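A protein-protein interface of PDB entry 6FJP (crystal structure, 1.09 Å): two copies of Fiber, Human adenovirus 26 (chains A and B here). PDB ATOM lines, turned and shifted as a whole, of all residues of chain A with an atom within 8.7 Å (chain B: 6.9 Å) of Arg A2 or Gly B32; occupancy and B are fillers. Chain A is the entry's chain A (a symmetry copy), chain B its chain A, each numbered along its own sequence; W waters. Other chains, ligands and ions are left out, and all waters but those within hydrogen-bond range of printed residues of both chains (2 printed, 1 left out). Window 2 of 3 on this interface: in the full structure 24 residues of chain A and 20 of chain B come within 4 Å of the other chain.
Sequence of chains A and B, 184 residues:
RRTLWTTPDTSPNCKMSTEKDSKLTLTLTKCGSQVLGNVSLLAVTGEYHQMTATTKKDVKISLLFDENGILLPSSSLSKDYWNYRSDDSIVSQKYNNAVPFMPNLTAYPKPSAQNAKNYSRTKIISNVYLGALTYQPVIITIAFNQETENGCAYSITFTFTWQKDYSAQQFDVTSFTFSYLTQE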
ATOM      1  N   ARG A   1     -12.353  -9.755   3.917  1.00  0.00           N
ATOM      2  CA  ARG A   1     -13.038 -11.043   3.643  1.00  0.00           C
ATOM      3  C   ARG A   1     -12.099 -12.235   3.696  1.00  0.00           C
ATOM      4  O   ARG A   1     -10.901 -12.128   3.983  1.00  0.00           O
ATOM      5  CB  ARG A   1     -13.871 -10.981   2.347  1.00  0.00           C
ATOM      6  CG  ARG A   1     -13.089 -10.951   1.050  1.00  0.00           C
ATOM      7  CD  ARG A   1     -13.170 -12.271   0.288  1.00  0.00           C
ATOM      8  NE  ARG A   1     -14.518 -12.461  -0.277  1.00  0.00           N
ATOM      9  CZ  ARG A   1     -15.358 -13.473  -0.024  1.00  0.00           C
ATOM     10  NH1 ARG A   1     -15.031 -14.494   0.774  1.00  0.00           N
ATOM     11  NH2 ARG A   1     -16.550 -13.483  -0.622  1.00  0.00           N
ATOM     12  N   ARG A   2     -12.691 -13.385   3.466  1.00  0.00           N
ATOM     13  CA  ARG A   2     -12.173 -14.607   3.963  1.00  0.00           C
ATOM     14  C   ARG A   2     -11.669 -15.602   2.943  1.00  0.00           C
ATOM     15  O   ARG A   2     -11.176 -16.597   3.380  1.00  0.00           O
ATOM     16  CB  ARG A   2     -13.153 -15.246   4.957  1.00  0.00           C
ATOM     17  CG  ARG A   2     -13.562 -14.364   6.138  1.00  0.00           C
ATOM     18  CD  ARG A   2     -14.675 -15.032   6.975  1.00  0.00           C
ATOM     19  NE  ARG A   2     -14.322 -16.380   7.482  1.00  0.00           N
ATOM     20  CZ  ARG A   2     -14.572 -17.574   6.903  1.00  0.00           C
ATOM     21  NH1 ARG A   2     -14.230 -18.709   7.543  1.00  0.00           N
ATOM     22  NH2 ARG A   2     -15.142 -17.682   5.704  1.00  0.00           N
ATOM     23  N   THR A   3     -11.680 -15.311   1.643  1.00  0.00           N
ATOM     24  CA  THR A   3     -11.058 -16.151   0.656  1.00  0.00           C
ATOM     25  C   THR A   3     -10.149 -15.355  -0.275  1.00  0.00           C
ATOM     26  O   THR A   3     -10.543 -14.348  -0.858  1.00  0.00           O
ATOM     27  CB  THR A   3     -12.093 -16.970  -0.172  1.00  0.00           C
ATOM     28  OG1 THR A   3     -12.638 -18.029   0.668  1.00  0.00           O
ATOM     29  CG2 THR A   3     -11.475 -17.608  -1.366  1.00  0.00           C
ATOM     30  N   LEU A   4      -8.930 -15.849  -0.453  1.00  0.00           N
ATOM     31  CA  LEU A   4      -8.028 -15.430  -1.544  1.00  0.00           C
ATOM     32  C   LEU A   4      -8.054 -16.523  -2.600  1.00  0.00           C
ATOM     33  O   LEU A   4      -7.965 -17.725  -2.266  1.00  0.00           O
ATOM     34  CB  LEU A   4      -6.589 -15.344  -1.107  1.00  0.00           C
ATOM     35  CG  LEU A   4      -6.189 -14.285  -0.150  1.00  0.00           C
ATOM     36  CD1 LEU A   4      -4.697 -14.429   0.198  1.00  0.00           C
ATOM     37  CD2 LEU A   4      -6.485 -12.925  -0.740  1.00  0.00           C
ATOM     38  N   TRP A   5      -8.155 -16.165  -3.892  1.00  0.00           N
ATOM     39  CA  TRP A   5      -8.151 -17.216  -4.894  1.00  0.00           C
ATOM     40  C   TRP A   5      -7.663 -16.692  -6.220  1.00  0.00           C
ATOM     41  O   TRP A   5      -7.474 -15.481  -6.458  1.00  0.00           O
ATOM     42  CB  TRP A   5      -9.535 -17.912  -5.013  1.00  0.00           C
ATOM     43  CG  TRP A   5     -10.636 -17.172  -5.642  1.00  0.00           C
ATOM     44  CD1 TRP A   5     -10.714 -15.859  -6.000  1.00  0.00           C
ATOM     45  CD2 TRP A   5     -11.878 -17.760  -5.999  1.00  0.00           C
ATOM     46  NE1 TRP A   5     -11.963 -15.593  -6.557  1.00  0.00           N
ATOM     47  CE2 TRP A   5     -12.677 -16.766  -6.558  1.00  0.00           C
ATOM     48  CE3 TRP A   5     -12.394 -19.067  -5.873  1.00  0.00           C
ATOM     49  CZ2 TRP A   5     -13.973 -17.034  -7.000  1.00  0.00           C
ATOM     50  CZ3 TRP A   5     -13.668 -19.318  -6.299  1.00  0.00           C
ATOM     51  CH2 TRP A   5     -14.438 -18.322  -6.867  1.00  0.00           C
ATOM     52  N   THR A  27      -7.361 -21.857  -4.008  1.00  0.00           N
ATOM     53  CA  THR A  27      -8.250 -21.169  -3.137  1.00  0.00           C
ATOM     54  C   THR A  27      -7.782 -21.307  -1.699  1.00  0.00           C
ATOM     55  O   THR A  27      -7.546 -22.452  -1.265  1.00  0.00           O
ATOM     56  CB  THR A  27      -9.665 -21.760  -3.287  1.00  0.00           C
ATOM     57  OG1 THR A  27     -10.039 -21.734  -4.672  1.00  0.00           O
ATOM     58  CG2 THR A  27     -10.681 -21.007  -2.478  1.00  0.00           C
ATOM     59  N   LEU A  28      -7.667 -20.193  -0.994  1.00  0.00           N
ATOM     60  CA  LEU A  28      -7.252 -20.149   0.406  1.00  0.00           C
ATOM     61  C   LEU A  28      -8.377 -19.534   1.188  1.00  0.00           C
ATOM     62  O   LEU A  28      -8.690 -18.345   1.006  1.00  0.00           O
ATOM     63  CB  LEU A  28      -5.941 -19.334   0.566  1.00  0.00           C
ATOM     64  CG  LEU A  28      -4.739 -19.827  -0.239  1.00  0.00           C
ATOM     65  CD1 LEU A  28      -3.570 -18.875   0.009  1.00  0.00           C
ATOM     66  CD2 LEU A  28      -4.373 -21.251   0.095  1.00  0.00           C
ATOM     67  N   THR A  29      -9.026 -20.306   2.070  1.00  0.00           N
ATOM     68  CA  THR A  29     -10.132 -19.821   2.864  1.00  0.00           C
ATOM     69  C   THR A  29      -9.736 -19.748   4.314  1.00  0.00           C
ATOM     70  O   THR A  29      -9.293 -20.753   4.902  1.00  0.00           O
ATOM     71  CB  THR A  29     -11.361 -20.714   2.697  1.00  0.00           C
ATOM     72  OG1 THR A  29     -11.731 -20.700   1.304  1.00  0.00           O
ATOM     73  CG2 THR A  29     -12.514 -20.200   3.506  1.00  0.00           C
ATOM     74  N   LYS A  30      -9.846 -18.583   4.907  1.00  0.00           N
ATOM     75  CA  LYS A  30      -9.451 -18.379   6.282  1.00  0.00           C
ATOM     76  C   LYS A  30     -10.488 -18.991   7.217  1.00  0.00           C
ATOM     77  O   LYS A  30     -11.641 -18.609   7.212  1.00  0.00           O
ATOM     78  CB  LYS A  30      -9.310 -16.874   6.528  1.00  0.00           C
ATOM     79  CG  LYS A  30      -9.163 -16.343   7.906  1.00  0.00           C
ATOM     80  CD  LYS A  30      -7.845 -16.784   8.408  1.00  0.00           C
ATOM     81  CE  LYS A  30      -7.491 -15.900   9.634  1.00  0.00           C
ATOM     82  NZ  LYS A  30      -6.169 -16.267  10.171  1.00  0.00           N
ATOM     83  N   CYS A  31     -10.040 -19.919   8.071  1.00  0.00           N
ATOM     84  CA  CYS A  31     -10.831 -20.574   9.095  1.00  0.00           C
ATOM     85  C   CYS A  31     -10.146 -20.353  10.461  1.00  0.00           C
ATOM     86  O   CYS A  31      -9.446 -21.273  10.965  1.00  0.00           O
ATOM     87  CB  CYS A  31     -10.896 -22.056   8.782  1.00  0.00           C
ATOM     88  SG  CYS A  31     -11.788 -22.464   7.277  1.00  0.00           S
ATOM     89  N   GLY A  32     -10.150 -19.127  10.926  1.00  0.00           N
ATOM     90  CA  GLY A  32      -9.485 -18.795  12.174  1.00  0.00           C
ATOM     91  C   GLY A  32      -7.993 -19.023  12.103  1.00  0.00           C
ATOM     92  O   GLY A  32      -7.326 -18.478  11.224  1.00  0.00           O
ATOM     93  N   GLN A  34      -6.325 -21.477  11.038  1.00  0.00           N
ATOM     94  CA  GLN A  34      -5.894 -22.227   9.869  1.00  0.00           C
ATOM     95  C   GLN A  34      -6.475 -21.625   8.594  1.00  0.00           C
ATOM     96  O   GLN A  34      -7.553 -21.054   8.657  1.00  0.00           O
ATOM     97  CB  GLN A  34      -6.300 -23.684   9.946  1.00  0.00           C
ATOM     98  CG  GLN A  34      -5.561 -24.425  11.055  1.00  0.00           C
ATOM     99  CD  GLN A  34      -6.041 -25.890  11.105  1.00  0.00           C
ATOM    100  OE1 GLN A  34      -5.783 -26.697  10.245  1.00  0.00           O
ATOM    101  NE2 GLN A  34      -6.749 -26.212  12.164  1.00  0.00           N
ATOM    102  N   VAL A  35      -5.768 -21.783   7.510  1.00  0.00           N
ATOM    103  CA  VAL A  35      -6.315 -21.651   6.192  1.00  0.00           C
ATOM    104  C   VAL A  35      -6.650 -23.041   5.693  1.00  0.00           C
ATOM    105  O   VAL A  35      -5.845 -23.976   5.815  1.00  0.00           O
ATOM    106  CB  VAL A  35      -5.334 -20.938   5.257  1.00  0.00           C
ATOM    107  CG1 VAL A  35      -5.616 -21.248   3.796  1.00  0.00           C
ATOM    108  CG2 VAL A  35      -5.370 -19.448   5.522  1.00  0.00           C
ATOM    109  N   LEU A  36      -7.849 -23.171   5.067  1.00  0.00           N
ATOM    110  CA  LEU A  36      -8.264 -24.338   4.318  1.00  0.00           C
ATOM    111  C   LEU A  36      -7.939 -24.079   2.851  1.00  0.00           C
ATOM    112  O   LEU A  36      -8.480 -23.104   2.264  1.00  0.00           O
ATOM    113  CB  LEU A  36      -9.744 -24.562   4.509  1.00  0.00           C
ATOM    114  CG  LEU A  36     -10.360 -25.743   3.788  1.00  0.00           C
ATOM    115  CD1 LEU A  36      -9.804 -27.086   4.260  1.00  0.00           C
ATOM    116  CD2 LEU A  36     -11.871 -25.726   3.943  1.00  0.00           C
ATOM    117  N   ASN A  83      -6.514 -12.536  -5.894  1.00  0.00           N
ATOM    118  CA  ASN A  83      -6.992 -11.540  -4.954  1.00  0.00           C
ATOM    119  C   ASN A  83      -8.205 -12.132  -4.174  1.00  0.00           C
ATOM    120  O   ASN A  83      -8.546 -13.343  -4.292  1.00  0.00           O
ATOM    121  CB  ASN A  83      -7.302 -10.225  -5.644  1.00  0.00           C
ATOM    122  CG  ASN A  83      -7.576  -9.104  -4.653  1.00  0.00           C
ATOM    123  OD1 ASN A  83      -6.756  -8.798  -3.753  1.00  0.00           O
ATOM    124  ND2 ASN A  83      -8.776  -8.702  -4.645  1.00  0.00           N
ATOM    125  N   TYR A  84      -8.760 -11.304  -3.293  1.00  0.00           N
ATOM    126  CA  TYR A  84      -9.937 -11.653  -2.546  1.00  0.00           C
ATOM    127  C   TYR A  84     -11.128 -12.015  -3.433  1.00  0.00           C
ATOM    128  O   TYR A  84     -11.336 -11.303  -4.461  1.00  0.00           O
ATOM    129  CB  TYR A  84     -10.221 -10.503  -1.566  1.00  0.00           C
ATOM    130  CG  TYR A  84      -9.279 -10.406  -0.393  1.00  0.00           C
ATOM    131  CD1 TYR A  84      -9.497 -11.196   0.722  1.00  0.00           C
ATOM    132  CD2 TYR A  84      -8.194  -9.508  -0.352  1.00  0.00           C
ATOM    133  CE1 TYR A  84      -8.680 -11.109   1.853  1.00  0.00           C
ATOM    134  CE2 TYR A  84      -7.344  -9.438   0.770  1.00  0.00           C
ATOM    135  CZ  TYR A  84      -7.595 -10.247   1.873  1.00  0.00           C
ATOM    136  OH  TYR A  84      -6.817 -10.223   3.027  1.00  0.00           O
ATOM    137  N   ARG A  85     -11.931 -13.029  -3.088  1.00  0.00           N
ATOM    138  CA  ARG A  85     -13.101 -13.454  -3.877  1.00  0.00           C
ATOM    139  C   ARG A  85     -14.142 -12.316  -3.941  1.00  0.00           C
ATOM    140  O   ARG A  85     -14.354 -11.581  -2.967  1.00  0.00           O
ATOM    141  CB  ARG A  85     -13.719 -14.823  -3.409  1.00  0.00           C
ATOM    142  CG  ARG A  85     -14.990 -15.298  -4.170  1.00  0.00           C
ATOM    143  CD  ARG A  85     -15.464 -16.757  -3.975  1.00  0.00           C
ATOM    144  NE  ARG A  85     -16.677 -17.066  -4.777  1.00  0.00           N
ATOM    145  CZ  ARG A  85     -17.286 -18.266  -4.860  1.00  0.00           C
ATOM    146  NH1 ARG A  85     -16.855 -19.338  -4.183  1.00  0.00           N
ATOM    147  NH2 ARG A  85     -18.343 -18.414  -5.646  1.00  0.00           N
ATOM    148  N   PRO A 100      -3.207 -12.428   7.653  1.00  0.00           N
ATOM    149  CA  PRO A 100      -3.927 -13.573   8.250  1.00  0.00           C
ATOM    150  C   PRO A 100      -4.038 -14.807   7.392  1.00  0.00           C
ATOM    151  O   PRO A 100      -4.512 -15.848   7.911  1.00  0.00           O
ATOM    152  CB  PRO A 100      -5.290 -12.993   8.593  1.00  0.00           C
ATOM    153  CG  PRO A 100      -5.000 -11.514   8.736  1.00  0.00           C
ATOM    154  CD  PRO A 100      -4.055 -11.236   7.604  1.00  0.00           C
ATOM    155  N   PHE A 101      -3.647 -14.754   6.135  1.00  0.00           N
ATOM    156  CA  PHE A 101      -3.575 -15.909   5.270  1.00  0.00           C
ATOM    157  C   PHE A 101      -2.176 -16.486   5.181  1.00  0.00           C
ATOM    158  O   PHE A 101      -1.981 -17.484   4.528  1.00  0.00           O
ATOM    159  CB  PHE A 101      -4.039 -15.563   3.857  1.00  0.00           C
ATOM    160  CG  PHE A 101      -5.499 -15.219   3.749  1.00  0.00           C
ATOM    161  CD1 PHE A 101      -5.968 -13.994   4.098  1.00  0.00           C
ATOM    162  CD2 PHE A 101      -6.412 -16.176   3.281  1.00  0.00           C
ATOM    163  CE1 PHE A 101      -7.309 -13.681   4.008  1.00  0.00           C
ATOM    164  CE2 PHE A 101      -7.746 -15.860   3.199  1.00  0.00           C
ATOM    165  CZ  PHE A 101      -8.175 -14.642   3.516  1.00  0.00           C
ATOM    166  N   ARG B   2     -25.253 -24.035   8.585  1.00  0.00           N
ATOM    167  CA  ARG B   2     -24.000 -24.244   7.957  1.00  0.00           C
ATOM    168  C   ARG B   2     -23.546 -25.676   7.790  1.00  0.00           C
ATOM    169  O   ARG B   2     -22.522 -25.837   7.201  1.00  0.00           O
ATOM    170  CB  ARG B   2     -22.917 -23.368   8.605  1.00  0.00           C
ATOM    171  CG  ARG B   2     -23.214 -21.868   8.635  1.00  0.00           C
ATOM    172  CD  ARG B   2     -22.153 -21.105   9.458  1.00  0.00           C
ATOM    173  NE  ARG B   2     -20.762 -21.310   8.986  1.00  0.00           N
ATOM    174  CZ  ARG B   2     -19.871 -22.231   9.410  1.00  0.00           C
ATOM    175  NH1 ARG B   2     -18.621 -22.231   8.907  1.00  0.00           N
ATOM    176  NH2 ARG B   2     -20.180 -23.162  10.312  1.00  0.00           N
ATOM    177  N   THR B  29     -19.886 -29.081   5.580  1.00  0.00           N
ATOM    178  CA  THR B  29     -19.896 -27.887   6.395  1.00  0.00           C
ATOM    179  C   THR B  29     -19.437 -26.704   5.586  1.00  0.00           C
ATOM    180  O   THR B  29     -18.338 -26.724   5.001  1.00  0.00           O
ATOM    181  CB  THR B  29     -19.010 -28.058   7.629  1.00  0.00           C
ATOM    182  OG1 THR B  29     -19.527 -29.163   8.395  1.00  0.00           O
ATOM    183  CG2 THR B  29     -19.034 -26.826   8.484  1.00  0.00           C
ATOM    184  N   LYS B  30     -20.256 -25.683   5.502  1.00  0.00           N
ATOM    185  CA  LYS B  30     -19.946 -24.512   4.714  1.00  0.00           C
ATOM    186  C   LYS B  30     -18.907 -23.661   5.434  1.00  0.00           C
ATOM    187  O   LYS B  30     -19.129 -23.192   6.531  1.00  0.00           O
ATOM    188  CB  LYS B  30     -21.240 -23.723   4.489  1.00  0.00           C
ATOM    189  CG  LYS B  30     -21.201 -22.348   3.933  1.00  0.00           C
ATOM    190  CD  LYS B  30     -20.747 -22.453   2.530  1.00  0.00           C
ATOM    191  CE  LYS B  30     -21.112 -21.123   1.818  1.00  0.00           C
ATOM    192  NZ  LYS B  30     -20.713 -21.170   0.401  1.00  0.00           N
ATOM    193  N   CYS B  31     -17.773 -23.419   4.763  1.00  0.00           N
ATOM    194  CA  CYS B  31     -16.686 -22.576   5.222  1.00  0.00           C
ATOM    195  C   CYS B  31     -16.428 -21.486   4.160  1.00  0.00           C
ATOM    196  O   CYS B  31     -15.468 -21.614   3.354  1.00  0.00           O
ATOM    197  CB  CYS B  31     -15.448 -23.435   5.395  1.00  0.00           C
ATOM    198  SG  CYS B  31     -15.568 -24.665   6.699  1.00  0.00           S
ATOM    199  N   GLY B  32     -17.365 -20.581   4.012  1.00  0.00           N
ATOM    200  CA  GLY B  32     -17.251 -19.542   3.003  1.00  0.00           C
ATOM    201  C   GLY B  32     -17.236 -20.108   1.602  1.00  0.00           C
ATOM    202  O   GLY B  32     -18.153 -20.834   1.220  1.00  0.00           O
ATOM    203  N   SER B  33     -16.175 -19.827   0.832  1.00  0.00           N
ATOM    204  CA  SER B  33     -16.006 -20.287  -0.563  1.00  0.00           C
ATOM    205  C   SER B  33     -15.796 -21.773  -0.751  1.00  0.00           C
ATOM    206  O   SER B  33     -15.697 -22.267  -1.884  1.00  0.00           O
ATOM    207  CB  SER B  33     -14.781 -19.579  -1.157  1.00  0.00           C
ATOM    208  OG  SER B  33     -15.059 -18.242  -1.506  1.00  0.00           O
ATOM    209  N   GLN B  34     -15.598 -22.494   0.354  1.00  0.00           N
ATOM    210  CA  GLN B  34     -15.419 -23.937   0.298  1.00  0.00           C
ATOM    211  C   GLN B  34     -16.405 -24.641   1.224  1.00  0.00           C
ATOM    212  O   GLN B  34     -16.782 -24.057   2.228  1.00  0.00           O
ATOM    213  CB  GLN B  34     -14.014 -24.352   0.680  1.00  0.00           C
ATOM    214  CG  GLN B  34     -12.984 -23.891  -0.346  1.00  0.00           C
ATOM    215  CD  GLN B  34     -11.574 -24.313   0.114  1.00  0.00           C
ATOM    216  OE1 GLN B  34     -11.203 -25.461   0.133  1.00  0.00           O
ATOM    217  NE2 GLN B  34     -10.786 -23.326   0.480  1.00  0.00           N
ATOM    218  N   VAL B  35     -16.764 -25.844   0.873  1.00  0.00           N
ATOM    219  CA  VAL B  35     -17.341 -26.787   1.785  1.00  0.00           C
ATOM    220  C   VAL B  35     -16.231 -27.696   2.268  1.00  0.00           C
ATOM    221  O   VAL B  35     -15.418 -28.192   1.475  1.00  0.00           O
ATOM    222  CB  VAL B  35     -18.468 -27.581   1.117  1.00  0.00           C
ATOM    223  CG1 VAL B  35     -18.727 -28.902   1.824  1.00  0.00           C
ATOM    224  CG2 VAL B  35     -19.721 -26.733   1.055  1.00  0.00           C
ATOM    225  N   PRO B 100     -25.535 -22.613  -1.725  1.00  0.00           N
ATOM    226  CA  PRO B 100     -24.175 -22.362  -1.201  1.00  0.00           C
ATOM    227  C   PRO B 100     -23.372 -23.581  -0.826  1.00  0.00           C
ATOM    228  O   PRO B 100     -22.166 -23.423  -0.515  1.00  0.00           O
ATOM    229  CB  PRO B 100     -24.419 -21.452  -0.009  1.00  0.00           C
ATOM    230  CG  PRO B 100     -25.745 -20.804  -0.344  1.00  0.00           C
ATOM    231  CD  PRO B 100     -26.548 -21.937  -0.915  1.00  0.00           C
ATOM    232  N   TYR B 180     -14.242 -28.533  -1.447  1.00  0.00           N
ATOM    233  CA  TYR B 180     -14.490 -28.116  -2.818  1.00  0.00           C
ATOM    234  C   TYR B 180     -15.013 -26.726  -2.834  1.00  0.00           C
ATOM    235  O   TYR B 180     -15.561 -26.206  -1.847  1.00  0.00           O
ATOM    236  CB  TYR B 180     -15.459 -29.064  -3.541  1.00  0.00           C
ATOM    237  CG  TYR B 180     -16.832 -29.199  -2.885  1.00  0.00           C
ATOM    238  CD1 TYR B 180     -17.889 -28.363  -3.247  1.00  0.00           C
ATOM    239  CD2 TYR B 180     -17.078 -30.175  -1.933  1.00  0.00           C
ATOM    240  CE1 TYR B 180     -19.123 -28.494  -2.671  1.00  0.00           C
ATOM    241  CE2 TYR B 180     -18.325 -30.322  -1.359  1.00  0.00           C
ATOM    242  CZ  TYR B 180     -19.360 -29.490  -1.734  1.00  0.00           C
ATOM    243  OH  TYR B 180     -20.566 -29.664  -1.095  1.00  0.00           O
ATOM    244  N   THR B 182     -17.428 -23.672  -3.818  1.00  0.00           N
ATOM    245  CA  THR B 182     -18.885 -23.618  -3.889  1.00  0.00           C
ATOM    246  C   THR B 182     -19.420 -22.612  -4.893  1.00  0.00           C
ATOM    247  O   THR B 182     -18.789 -21.605  -5.249  1.00  0.00           O
ATOM    248  CB  THR B 182     -19.495 -23.304  -2.521  1.00  0.00           C
ATOM    249  OG1 THR B 182     -19.082 -22.000  -2.127  1.00  0.00           O
ATOM    250  CG2 THR B 182     -19.072 -24.255  -1.421  1.00  0.00           C
ATOM    251  N   GLN B 183     -20.675 -22.902  -5.289  1.00  0.00           N
ATOM    252  CA  GLN B 183     -21.525 -21.952  -5.962  1.00  0.00           C
ATOM    253  C   GLN B 183     -22.051 -20.918  -4.845  1.00  0.00           C
ATOM    254  O   GLN B 183     -21.985 -21.233  -3.623  1.00  0.00           O
ATOM    255  CB  GLN B 183     -22.698 -22.755  -6.609  1.00  0.00           C
ATOM    256  CG  GLN B 183     -23.474 -22.025  -7.659  1.00  0.00           C
ATOM    257  CD  GLN B 183     -22.786 -21.987  -9.022  1.00  0.00           C
ATOM    258  OE1 GLN B 183     -21.656 -22.485  -9.214  1.00  0.00           O
ATOM    259  NE2 GLN B 183     -23.429 -21.264  -9.979  1.00  0.00           N
ATOM    260  N   GLU B 184     -22.664 -19.809  -5.234  1.00  0.00           N
ATOM    261  CA  GLU B 184     -23.427 -18.956  -4.278  1.00  0.00           C
ATOM    262  C   GLU B 184     -24.788 -18.640  -4.864  1.00  0.00           C
ATOM    263  O   GLU B 184     -25.780 -18.357  -4.154  1.00  0.00           O
ATOM    264  CB  GLU B 184     -22.660 -17.669  -3.937  1.00  0.00           C
ATOM    265  CG  GLU B 184     -21.325 -17.909  -3.220  1.00  0.00           C
ATOM    266  CD  GLU B 184     -21.472 -18.537  -1.843  1.00  0.00           C
ATOM    267  OE1 GLU B 184     -22.565 -18.456  -1.219  1.00  0.00           O
ATOM    268  OE2 GLU B 184     -20.475 -19.114  -1.379  1.00  0.00           O
ATOM    269  OXT GLU B 184     -24.910 -18.732  -6.087  1.00  0.00           O
HETATM  270  O   HOH W   1     -17.210 -16.501  -0.941  1.00  0.00           O
HETATM  271  O   HOH W   2     -14.990 -17.127   1.583  1.00  0.00           O
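The side-chain amide nitrogen of Gln B34 lies within hydrogen-bond range of the backbone carbonyl oxygen of Leu A36 (2.9 Å).
OG of Ser B33 sits close to OG1 of Thr A3 (3.3 Å).
NH1 of Arg A85 lies close to OG of Ser B33, at 3.4 Å.
The side-chain amide nitrogen (NE2) of Gln B34 lies within hydrogen-bond range of the side-chain hydroxyl (OG1) of Thr A29 (2.9 Å).
O of Thr B182 is in hydrogen-bond range of NH1 of Arg A85 (3.2 Å).
The backbone carbonyl oxygen (O) of Gly B32 lies within hydrogen-bond range of the side-chain amino group (NZ) of Lys B30, at 2.7 Å.
O of Ser B33 sits at hydrogen-bond distance from N of Thr B182 (3.0 Å).
The side-chain amino group (NZ) of Lys B30 is in hydrogen-bond range of the side-chain hydroxyl (OG1) of Thr B182 (3.1 Å).
N of Arg A85 sits at hydrogen-bond distance from O of Thr A3.
OG1 of Thr A29 sits at hydrogen-bond distance from OG1 of Thr A3 (2.9 Å).
O of Lys A30 is in hydrogen-bond range of NH1 of Arg A2 (2.6 Å).
Gly B32 touches Arg A2 (CA to NH2, 3.9 Å).
NE2 of Gln B34 touches CG2 of Thr A27, 3.8 Å away.
Thr A29 touches Cys B31.
NH2 of Arg A85 touches CG of Glu B184 (3.9 Å).
Arg A2 touches one residue of chain B.
Of chain A, only Arg A2 (3.9 Å) comes within 4 Å of Gly B32.
Of the printed residues of chain B, Leu A36 touches Gln B34 (2.9 Å).
Printed residues of chain A within 4 Å of Ser B33: Thr A3 and Arg A85.
Of the printed residues of chain B, Thr A3 touches Ser B33.
Of the printed residues of chain A, Thr B182 touches Arg A85.
Of the printed residues of chain B, Thr A27 touches Gln B34.
The nearest residue of chain B that does not touch Arg A2 is Cys B31 (4.3 Å).
Of the 19 printed residues of chain A, 6 touch a printed residue of chain B.
Hydrophobic or aromatic side chains of chain A that line the printed part of chain B: Leu A36.
Printed residues of chain B that touch a printed residue of chain A: Cys B31, Gly B32, Ser B33, Gln B34, Thr B182 and Glu B184.
Arg A2 touches Gly B32, but with the chains exchanged Gly A32 does not touch Arg B2 (9.2 Å).
Thr A29 touches Cys B31, but with the chains exchanged Cys A31 does not touch Thr B29 (8.1 Å).
Thr A29 touches Gln B34, but with the chains exchanged Gln A34 does not touch Thr B29 (12.7 Å).
Water W2 lies within hydrogen-bond range of the side-chain hydroxyl of Thr A3, the guanidinium group of Arg A1 and the backbone NH of Ser B33.
Water W1 lies within hydrogen-bond range of OG of Ser B33 (2.8 Å) and NH2 of Arg A1 (3.1 Å).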
